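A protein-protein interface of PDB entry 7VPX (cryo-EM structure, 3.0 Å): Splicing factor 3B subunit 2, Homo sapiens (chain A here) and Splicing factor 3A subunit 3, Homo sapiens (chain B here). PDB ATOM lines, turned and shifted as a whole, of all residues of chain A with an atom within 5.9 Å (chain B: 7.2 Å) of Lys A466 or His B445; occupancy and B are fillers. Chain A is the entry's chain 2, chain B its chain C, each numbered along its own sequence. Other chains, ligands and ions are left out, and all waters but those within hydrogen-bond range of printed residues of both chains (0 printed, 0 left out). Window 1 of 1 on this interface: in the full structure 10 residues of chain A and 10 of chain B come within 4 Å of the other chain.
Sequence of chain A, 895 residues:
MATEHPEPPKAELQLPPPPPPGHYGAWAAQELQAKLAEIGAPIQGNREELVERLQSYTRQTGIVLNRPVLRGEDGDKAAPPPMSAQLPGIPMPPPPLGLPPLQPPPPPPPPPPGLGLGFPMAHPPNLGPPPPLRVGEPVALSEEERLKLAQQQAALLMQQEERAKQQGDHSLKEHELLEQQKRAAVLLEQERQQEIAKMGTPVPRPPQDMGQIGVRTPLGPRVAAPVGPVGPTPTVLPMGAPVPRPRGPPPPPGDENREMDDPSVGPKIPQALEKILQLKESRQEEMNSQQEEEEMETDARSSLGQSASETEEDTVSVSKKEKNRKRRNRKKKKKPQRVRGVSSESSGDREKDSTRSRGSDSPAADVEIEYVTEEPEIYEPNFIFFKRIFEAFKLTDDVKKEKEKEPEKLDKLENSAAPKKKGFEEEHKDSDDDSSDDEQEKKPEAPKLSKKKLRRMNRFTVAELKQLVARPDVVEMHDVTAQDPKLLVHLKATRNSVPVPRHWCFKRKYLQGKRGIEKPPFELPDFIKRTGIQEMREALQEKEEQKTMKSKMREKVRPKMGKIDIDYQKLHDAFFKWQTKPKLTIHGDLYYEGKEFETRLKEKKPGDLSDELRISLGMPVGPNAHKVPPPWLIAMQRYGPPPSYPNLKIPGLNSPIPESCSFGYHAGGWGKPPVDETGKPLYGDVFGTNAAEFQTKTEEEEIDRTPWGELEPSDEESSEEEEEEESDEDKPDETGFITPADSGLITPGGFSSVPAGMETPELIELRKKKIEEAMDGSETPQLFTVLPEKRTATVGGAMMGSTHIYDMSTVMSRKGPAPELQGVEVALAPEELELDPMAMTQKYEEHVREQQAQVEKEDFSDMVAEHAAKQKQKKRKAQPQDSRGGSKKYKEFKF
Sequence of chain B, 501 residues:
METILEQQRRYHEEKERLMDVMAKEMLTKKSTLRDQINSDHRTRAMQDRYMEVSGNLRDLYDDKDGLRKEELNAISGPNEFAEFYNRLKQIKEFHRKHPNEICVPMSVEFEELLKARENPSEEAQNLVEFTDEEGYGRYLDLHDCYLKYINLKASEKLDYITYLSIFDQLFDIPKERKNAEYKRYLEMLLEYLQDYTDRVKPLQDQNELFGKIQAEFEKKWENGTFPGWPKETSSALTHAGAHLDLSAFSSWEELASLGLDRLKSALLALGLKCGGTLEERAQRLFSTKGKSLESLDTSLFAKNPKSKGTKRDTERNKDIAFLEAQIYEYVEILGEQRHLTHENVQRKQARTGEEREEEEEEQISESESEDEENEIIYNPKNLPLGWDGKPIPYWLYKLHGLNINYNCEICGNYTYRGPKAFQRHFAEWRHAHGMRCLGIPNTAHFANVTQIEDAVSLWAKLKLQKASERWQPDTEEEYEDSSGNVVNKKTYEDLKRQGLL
O of Ala B447 is in hydrogen-bond range of NZ of Lys A466 (2.6 Å).
N of Leu B458 lies close to NE2 of Gln A467 (3.2 Å).
The backbone carbonyl oxygen (O) of Gln A467 sits close to the side-chain amino group (NZ) of Lys B461, at 3.3 Å.
The side-chain amino group (NZ) of Lys B461 is in hydrogen-bond range of the backbone carbonyl oxygen (O) of Val A469 (3.2 Å).
Of the printed residues of chain B, Val A462 touches Asn B448.
Of chain B, only His B445, Ala B447, Leu B458 and Lys B461 come within 4 Å of Lys A466.
Printed residues of chain B within 4 Å of Gln A467: Leu B458 (3.2 Å) and Lys B461 (3.1 Å).
Printed residues of chain B within 4 Å of Val A469: Lys B461.
Printed residues of chain A within 4 Å of Ala B444: Asp A473.
Of the printed residues of chain A, Lys B461 touches Lys A466 (3.7 Å), Gln A467 (3.1 Å) and Val A469 (3.2 Å).
Asn B448 touches Val A462 (O to CG1, 3.6 Å).
His B445 touches Lys A466 (O to CE, 3.1 Å).
O of Lys A466 touches CD1 of Leu B458, at 3.6 Å.
Lys A466 touches Lys B461 (O to CE, 3.7 Å).
His B445 touches Pro A472.
C of Ala B444 touches CB of Asp A473 (3.8 Å).
OD2 of Asp A473 touches CE1 of His B445, at 3.6 Å.
Printed residues of chain B that touch a printed residue of chain A: Ala B444, His B445, Ala B447, Asn B448, Leu B458 and Lys B461.
Hydrophobic or aromatic side chains of chain B that line the printed part of chain A: His B445 and Leu B458.
Of the 14 printed residues of chain A, 6 touch a printed residue of chain B.
Printed residues of chain A that touch a printed residue of chain B: Val A462, Lys A466, Gln A467, Val A469, Pro A472 and Asp A473.
Among the printed residues, 11 pairs touch across the chains.
Among the printed residues, no Asp or Glu carboxylate lies within 4 Å of a Lys or Arg side-chain nitrogen of the other chain.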
ATOM      1  N   THR A 461      14.343 -17.429  30.969  1.00  0.00           N
ATOM      2  CA  THR A 461      12.946 -17.805  31.087  1.00  0.00           C
ATOM      3  C   THR A 461      12.161 -17.183  29.938  1.00  0.00           C
ATOM      4  O   THR A 461      12.639 -16.281  29.245  1.00  0.00           O
ATOM      5  CB  THR A 461      12.367 -17.361  32.432  1.00  0.00           C
ATOM      6  OG1 THR A 461      12.153 -15.945  32.424  1.00  0.00           O
ATOM      7  CG2 THR A 461      13.308 -17.724  33.570  1.00  0.00           C
ATOM      8  N   VAL A 462      10.944 -17.686  29.727  1.00  0.00           N
ATOM      9  CA  VAL A 462      10.141 -17.221  28.600  1.00  0.00           C
ATOM     10  C   VAL A 462       9.878 -15.726  28.707  1.00  0.00           C
ATOM     11  O   VAL A 462      10.033 -14.981  27.733  1.00  0.00           O
ATOM     12  CB  VAL A 462       8.831 -18.025  28.509  1.00  0.00           C
ATOM     13  CG1 VAL A 462       7.869 -17.365  27.543  1.00  0.00           C
ATOM     14  CG2 VAL A 462       9.121 -19.447  28.075  1.00  0.00           C
ATOM     15  N   ALA A 463       9.500 -15.257  29.898  1.00  0.00           N
ATOM     16  CA  ALA A 463       9.199 -13.839  30.070  1.00  0.00           C
ATOM     17  C   ALA A 463      10.461 -12.991  29.986  1.00  0.00           C
ATOM     18  O   ALA A 463      10.419 -11.847  29.524  1.00  0.00           O
ATOM     19  CB  ALA A 463       8.487 -13.612  31.401  1.00  0.00           C
ATOM     20  N   GLU A 464      11.595 -13.534  30.436  1.00  0.00           N
ATOM     21  CA  GLU A 464      12.846 -12.790  30.356  1.00  0.00           C
ATOM     22  C   GLU A 464      13.311 -12.640  28.914  1.00  0.00           C
ATOM     23  O   GLU A 464      13.802 -11.578  28.518  1.00  0.00           O
ATOM     24  CB  GLU A 464      13.918 -13.478  31.199  1.00  0.00           C
ATOM     25  CG  GLU A 464      15.306 -12.876  31.054  1.00  0.00           C
ATOM     26  CD  GLU A 464      16.333 -13.576  31.920  1.00  0.00           C
ATOM     27  OE1 GLU A 464      15.975 -14.573  32.583  1.00  0.00           O
ATOM     28  OE2 GLU A 464      17.500 -13.128  31.940  1.00  0.00           O
ATOM     29  N   LEU A 465      13.163 -13.695  28.110  1.00  0.00           N
ATOM     30  CA  LEU A 465      13.562 -13.615  26.708  1.00  0.00           C
ATOM     31  C   LEU A 465      12.566 -12.791  25.903  1.00  0.00           C
ATOM     32  O   LEU A 465      12.933 -12.161  24.903  1.00  0.00           O
ATOM     33  CB  LEU A 465      13.716 -15.020  26.125  1.00  0.00           C
ATOM     34  CG  LEU A 465      13.847 -15.178  24.609  1.00  0.00           C
ATOM     35  CD1 LEU A 465      15.246 -14.807  24.144  1.00  0.00           C
ATOM     36  CD2 LEU A 465      13.509 -16.598  24.190  1.00  0.00           C
ATOM     37  N   LYS A 466      11.300 -12.771  26.329  1.00  0.00           N
ATOM     38  CA  LYS A 466      10.307 -11.945  25.652  1.00  0.00           C
ATOM     39  C   LYS A 466      10.618 -10.463  25.821  1.00  0.00           C
ATOM     40  O   LYS A 466      10.190  -9.634  25.011  1.00  0.00           O
ATOM     41  CB  LYS A 466       8.911 -12.266  26.186  1.00  0.00           C
ATOM     42  CG  LYS A 466       8.254 -13.477  25.550  1.00  0.00           C
ATOM     43  CD  LYS A 466       6.742 -13.394  25.636  1.00  0.00           C
ATOM     44  CE  LYS A 466       6.075 -14.416  24.735  1.00  0.00           C
ATOM     45  NZ  LYS A 466       6.001 -15.765  25.346  1.00  0.00           N
ATOM     46  N   GLN A 467      11.364 -10.113  26.872  1.00  0.00           N
ATOM     47  CA  GLN A 467      11.704  -8.715  27.118  1.00  0.00           C
ATOM     48  C   GLN A 467      12.879  -8.265  26.259  1.00  0.00           C
ATOM     49  O   GLN A 467      13.067  -7.065  26.030  1.00  0.00           O
ATOM     50  CB  GLN A 467      12.022  -8.506  28.598  1.00  0.00           C
ATOM     51  CG  GLN A 467      10.808  -8.496  29.504  1.00  0.00           C
ATOM     52  CD  GLN A 467      10.291  -7.098  29.758  1.00  0.00           C
ATOM     53  OE1 GLN A 467      11.053  -6.133  29.751  1.00  0.00           O
ATOM     54  NE2 GLN A 467       8.991  -6.981  29.985  1.00  0.00           N
ATOM     55  N   LEU A 468      13.698  -9.209  25.793  1.00  0.00           N
ATOM     56  CA  LEU A 468      14.899  -8.839  25.052  1.00  0.00           C
ATOM     57  C   LEU A 468      14.624  -8.706  23.558  1.00  0.00           C
ATOM     58  O   LEU A 468      15.262  -7.899  22.874  1.00  0.00           O
ATOM     59  CB  LEU A 468      16.003  -9.864  25.305  1.00  0.00           C
ATOM     60  CG  LEU A 468      16.610  -9.871  26.708  1.00  0.00           C
ATOM     61  CD1 LEU A 468      17.954 -10.580  26.708  1.00  0.00           C
ATOM     62  CD2 LEU A 468      16.751  -8.453  27.239  1.00  0.00           C
ATOM     63  N   VAL A 469      13.681  -9.490  23.035  1.00  0.00           N
ATOM     64  CA  VAL A 469      13.514  -9.599  21.592  1.00  0.00           C
ATOM     65  C   VAL A 469      12.592  -8.502  21.077  1.00  0.00           C
ATOM     66  O   VAL A 469      11.751  -7.966  21.814  1.00  0.00           O
ATOM     67  CB  VAL A 469      12.982 -10.994  21.225  1.00  0.00           C
ATOM     68  CG1 VAL A 469      13.929 -12.060  21.740  1.00  0.00           C
ATOM     69  CG2 VAL A 469      11.586 -11.198  21.786  1.00  0.00           C
ATOM     70  N   ARG A 471      10.365  -8.964  18.775  1.00  0.00           N
ATOM     71  CA  ARG A 471       9.082  -9.566  18.441  1.00  0.00           C
ATOM     72  C   ARG A 471       8.775 -10.692  19.416  1.00  0.00           C
ATOM     73  O   ARG A 471       9.208 -11.832  19.193  1.00  0.00           O
ATOM     74  CB  ARG A 471       9.090 -10.086  17.007  1.00  0.00           C
ATOM     75  CG  ARG A 471       7.717 -10.120  16.376  1.00  0.00           C
ATOM     76  CD  ARG A 471       7.718  -9.562  14.971  1.00  0.00           C
ATOM     77  NE  ARG A 471       6.372  -9.546  14.408  1.00  0.00           N
ATOM     78  CZ  ARG A 471       5.771 -10.607  13.882  1.00  0.00           C
ATOM     79  NH1 ARG A 471       4.543 -10.504  13.392  1.00  0.00           N
ATOM     80  NH2 ARG A 471       6.397 -11.776  13.845  1.00  0.00           N
ATOM     81  N   PRO A 472       8.038 -10.429  20.499  1.00  0.00           N
ATOM     82  CA  PRO A 472       7.865 -11.466  21.526  1.00  0.00           C
ATOM     83  C   PRO A 472       6.823 -12.517  21.183  1.00  0.00           C
ATOM     84  O   PRO A 472       6.804 -13.572  21.827  1.00  0.00           O
ATOM     85  CB  PRO A 472       7.457 -10.659  22.766  1.00  0.00           C
ATOM     86  CG  PRO A 472       6.816  -9.437  22.219  1.00  0.00           C
ATOM     87  CD  PRO A 472       7.504  -9.125  20.922  1.00  0.00           C
ATOM     88  N   ASP A 473       5.964 -12.284  20.189  1.00  0.00           N
ATOM     89  CA  ASP A 473       4.866 -13.217  19.953  1.00  0.00           C
ATOM     90  C   ASP A 473       5.323 -14.436  19.156  1.00  0.00           C
ATOM     91  O   ASP A 473       4.542 -15.368  18.937  1.00  0.00           O
ATOM     92  CB  ASP A 473       3.714 -12.512  19.237  1.00  0.00           C
ATOM     93  CG  ASP A 473       4.175 -11.708  18.046  1.00  0.00           C
ATOM     94  OD1 ASP A 473       5.385 -11.422  17.958  1.00  0.00           O
ATOM     95  OD2 ASP A 473       3.330 -11.362  17.194  1.00  0.00           O
ATOM     96  N   VAL A 475       8.009 -16.089  20.239  1.00  0.00           N
ATOM     97  CA  VAL A 475       8.676 -16.913  21.240  1.00  0.00           C
ATOM     98  C   VAL A 475       7.720 -17.995  21.725  1.00  0.00           C
ATOM     99  O   VAL A 475       6.518 -17.757  21.903  1.00  0.00           O
ATOM    100  CB  VAL A 475       9.176 -16.035  22.400  1.00  0.00           C
ATOM    101  CG1 VAL A 475       9.835 -16.879  23.479  1.00  0.00           C
ATOM    102  CG2 VAL A 475      10.144 -14.985  21.885  1.00  0.00           C
ATOM    103  N   GLU A 476       8.252 -19.197  21.943  1.00  0.00           N
ATOM    104  CA  GLU A 476       7.436 -20.339  22.329  1.00  0.00           C
ATOM    105  C   GLU A 476       8.055 -21.034  23.534  1.00  0.00           C
ATOM    106  O   GLU A 476       9.105 -20.637  24.042  1.00  0.00           O
ATOM    107  CB  GLU A 476       7.269 -21.323  21.165  1.00  0.00           C
ATOM    108  CG  GLU A 476       6.027 -21.066  20.328  1.00  0.00           C
ATOM    109  CD  GLU A 476       6.292 -21.180  18.843  1.00  0.00           C
ATOM    110  OE1 GLU A 476       6.991 -22.128  18.432  1.00  0.00           O
ATOM    111  OE2 GLU A 476       5.800 -20.319  18.082  1.00  0.00           O
ATOM    112  N   ASN B 442      -5.738 -10.186  25.643  1.00  0.00           N
ATOM    113  CA  ASN B 442      -5.158 -11.495  25.376  1.00  0.00           C
ATOM    114  C   ASN B 442      -4.711 -11.592  23.923  1.00  0.00           C
ATOM    115  O   ASN B 442      -5.537 -11.644  23.007  1.00  0.00           O
ATOM    116  CB  ASN B 442      -6.171 -12.595  25.687  1.00  0.00           C
ATOM    117  CG  ASN B 442      -5.746 -13.466  26.849  1.00  0.00           C
ATOM    118  OD1 ASN B 442      -4.783 -13.159  27.550  1.00  0.00           O
ATOM    119  ND2 ASN B 442      -6.461 -14.564  27.056  1.00  0.00           N
ATOM    120  N   THR B 443      -3.399 -11.614  23.713  1.00  0.00           N
ATOM    121  CA  THR B 443      -2.844 -11.739  22.372  1.00  0.00           C
ATOM    122  C   THR B 443      -1.752 -12.797  22.401  1.00  0.00           C
ATOM    123  O   THR B 443      -1.437 -13.365  23.448  1.00  0.00           O
ATOM    124  CB  THR B 443      -2.301 -10.400  21.858  1.00  0.00           C
ATOM    125  OG1 THR B 443      -1.709  -9.675  22.941  1.00  0.00           O
ATOM    126  CG2 THR B 443      -3.420  -9.568  21.247  1.00  0.00           C
ATOM    127  N   ALA B 444      -1.176 -13.057  21.225  1.00  0.00           N
ATOM    128  CA  ALA B 444      -0.134 -14.072  21.127  1.00  0.00           C
ATOM    129  C   ALA B 444       1.132 -13.635  21.851  1.00  0.00           C
ATOM    130  O   ALA B 444       1.963 -14.471  22.223  1.00  0.00           O
ATOM    131  CB  ALA B 444       0.164 -14.379  19.660  1.00  0.00           C
ATOM    132  N   HIS B 445       1.298 -12.325  22.059  1.00  0.00           N
ATOM    133  CA  HIS B 445       2.456 -11.836  22.797  1.00  0.00           C
ATOM    134  C   HIS B 445       2.449 -12.340  24.234  1.00  0.00           C
ATOM    135  O   HIS B 445       3.500 -12.676  24.788  1.00  0.00           O
ATOM    136  CB  HIS B 445       2.493 -10.308  22.779  1.00  0.00           C
ATOM    137  CG  HIS B 445       2.339  -9.709  21.414  1.00  0.00           C
ATOM    138  ND1 HIS B 445       3.373  -9.072  20.764  1.00  0.00           N
ATOM    139  CD2 HIS B 445       1.271  -9.637  20.586  1.00  0.00           C
ATOM    140  CE1 HIS B 445       2.950  -8.640  19.589  1.00  0.00           C
ATOM    141  NE2 HIS B 445       1.679  -8.970  19.456  1.00  0.00           N
ATOM    142  N   PHE B 446       1.274 -12.388  24.859  1.00  0.00           N
ATOM    143  CA  PHE B 446       1.156 -12.827  26.249  1.00  0.00           C
ATOM    144  C   PHE B 446       0.758 -14.302  26.293  1.00  0.00           C
ATOM    145  O   PHE B 446      -0.310 -14.687  26.774  1.00  0.00           O
ATOM    146  CB  PHE B 446       0.172 -11.947  27.005  1.00  0.00           C
ATOM    147  CG  PHE B 446       0.584 -10.508  27.073  1.00  0.00           C
ATOM    148  CD1 PHE B 446       1.518 -10.088  28.005  1.00  0.00           C
ATOM    149  CD2 PHE B 446       0.053  -9.577  26.196  1.00  0.00           C
ATOM    150  CE1 PHE B 446       1.907  -8.765  28.068  1.00  0.00           C
ATOM    151  CE2 PHE B 446       0.438  -8.256  26.254  1.00  0.00           C
ATOM    152  CZ  PHE B 446       1.365  -7.849  27.191  1.00  0.00           C
ATOM    153  N   ALA B 447       1.653 -15.133  25.772  1.00  0.00           N
ATOM    154  CA  ALA B 447       1.521 -16.577  25.847  1.00  0.00           C
ATOM    155  C   ALA B 447       2.732 -17.139  26.573  1.00  0.00           C
ATOM    156  O   ALA B 447       3.837 -16.598  26.486  1.00  0.00           O
ATOM    157  CB  ALA B 447       1.388 -17.209  24.455  1.00  0.00           C
ATOM    158  N   ASN B 448       2.503 -18.226  27.311  1.00  0.00           N
ATOM    159  CA  ASN B 448       3.527 -18.854  28.147  1.00  0.00           C
ATOM    160  C   ASN B 448       4.050 -17.901  29.220  1.00  0.00           C
ATOM    161  O   ASN B 448       5.112 -18.126  29.805  1.00  0.00           O
ATOM    162  CB  ASN B 448       4.683 -19.403  27.306  1.00  0.00           C
ATOM    163  CG  ASN B 448       4.207 -20.289  26.172  1.00  0.00           C
ATOM    164  OD1 ASN B 448       4.014 -19.830  25.047  1.00  0.00           O
ATOM    165  ND2 ASN B 448       4.014 -21.568  26.464  1.00  0.00           N
ATOM    166  N   VAL B 449       3.310 -16.826  29.485  1.00  0.00           N
ATOM    167  CA  VAL B 449       3.620 -15.887  30.557  1.00  0.00           C
ATOM    168  C   VAL B 449       2.598 -16.092  31.666  1.00  0.00           C
ATOM    169  O   VAL B 449       1.398 -15.877  31.460  1.00  0.00           O
ATOM    170  CB  VAL B 449       3.607 -14.436  30.050  1.00  0.00           C
ATOM    171  CG1 VAL B 449       3.657 -13.465  31.220  1.00  0.00           C
ATOM    172  CG2 VAL B 449       4.770 -14.197  29.103  1.00  0.00           C
ATOM    173  N   LEU B 458       5.816  -6.500  30.390  1.00  0.00           N
ATOM    174  CA  LEU B 458       5.791  -6.723  28.950  1.00  0.00           C
ATOM    175  C   LEU B 458       4.711  -5.877  28.289  1.00  0.00           C
ATOM    176  O   LEU B 458       4.860  -5.450  27.137  1.00  0.00           O
ATOM    177  CB  LEU B 458       5.582  -8.207  28.652  1.00  0.00           C
ATOM    178  CG  LEU B 458       5.814  -8.650  27.207  1.00  0.00           C
ATOM    179  CD1 LEU B 458       7.303  -8.793  26.934  1.00  0.00           C
ATOM    180  CD2 LEU B 458       5.088  -9.951  26.923  1.00  0.00           C
ATOM    181  N   LYS B 461       6.227  -2.494  27.903  1.00  0.00           N
ATOM    182  CA  LYS B 461       7.150  -2.527  26.771  1.00  0.00           C
ATOM    183  C   LYS B 461       6.411  -2.455  25.439  1.00  0.00           C
ATOM    184  O   LYS B 461       6.775  -1.663  24.559  1.00  0.00           O
ATOM    185  CB  LYS B 461       8.003  -3.791  26.831  1.00  0.00           C
ATOM    186  CG  LYS B 461       9.016  -3.898  25.709  1.00  0.00           C
ATOM    187  CD  LYS B 461      10.169  -4.802  26.090  1.00  0.00           C
ATOM    188  CE  LYS B 461      10.260  -5.982  25.133  1.00  0.00           C
ATOM    189  NZ  LYS B 461      11.009  -5.648  23.890  1.00  0.00           N
ATOM    190  N   LEU B 462       5.387  -3.294  25.265  1.00  0.00           N
ATOM    191  CA  LEU B 462       4.649  -3.315  24.006  1.00  0.00           C
ATOM    192  C   LEU B 462       3.929  -1.997  23.767  1.00  0.00           C
ATOM    193  O   LEU B 462       3.864  -1.513  22.629  1.00  0.00           O
ATOM    194  CB  LEU B 462       3.657  -4.475  24.004  1.00  0.00           C
ATOM    195  CG  LEU B 462       4.223  -5.842  23.612  1.00  0.00           C
ATOM    196  CD1 LEU B 462       3.174  -6.919  23.807  1.00  0.00           C
ATOM    197  CD2 LEU B 462       4.726  -5.830  22.176  1.00  0.00           C
ATOM    198  N   GLN B 465       6.559   0.520  22.598  1.00  0.00           N
ATOM    199  CA  GLN B 465       6.925   0.213  21.215  1.00  0.00           C
ATOM    200  C   GLN B 465       5.862   0.664  20.220  1.00  0.00           C
ATOM    201  O   GLN B 465       6.158   1.439  19.298  1.00  0.00           O
ATOM    202  CB  GLN B 465       7.155  -1.291  21.067  1.00  0.00           C
ATOM    203  CG  GLN B 465       7.984  -1.689  19.860  1.00  0.00           C
ATOM    204  CD  GLN B 465       7.857  -3.162  19.537  1.00  0.00           C
ATOM    205  OE1 GLN B 465       7.416  -3.535  18.450  1.00  0.00           O
ATOM    206  NE2 GLN B 465       8.236  -4.013  20.485  1.00  0.00           N
ATOM    207  N   LYS B 466       4.623   0.195  20.388  1.00  0.00           N
ATOM    208  CA  LYS B 466       3.581   0.520  19.423  1.00  0.00           C
ATOM    209  C   LYS B 466       3.292   2.014  19.401  1.00  0.00           C
ATOM    210  O   LYS B 466       3.254   2.624  18.327  1.00  0.00           O
ATOM    211  CB  LYS B 466       2.312  -0.281  19.716  1.00  0.00           C
ATOM    212  CG  LYS B 466       2.142  -1.481  18.795  1.00  0.00           C
ATOM    213  CD  LYS B 466       0.955  -2.348  19.186  1.00  0.00           C
ATOM    214  CE  LYS B 466       1.062  -2.844  20.619  1.00  0.00           C
ATOM    215  NZ  LYS B 466      -0.257  -3.310  21.135  1.00  0.00           N
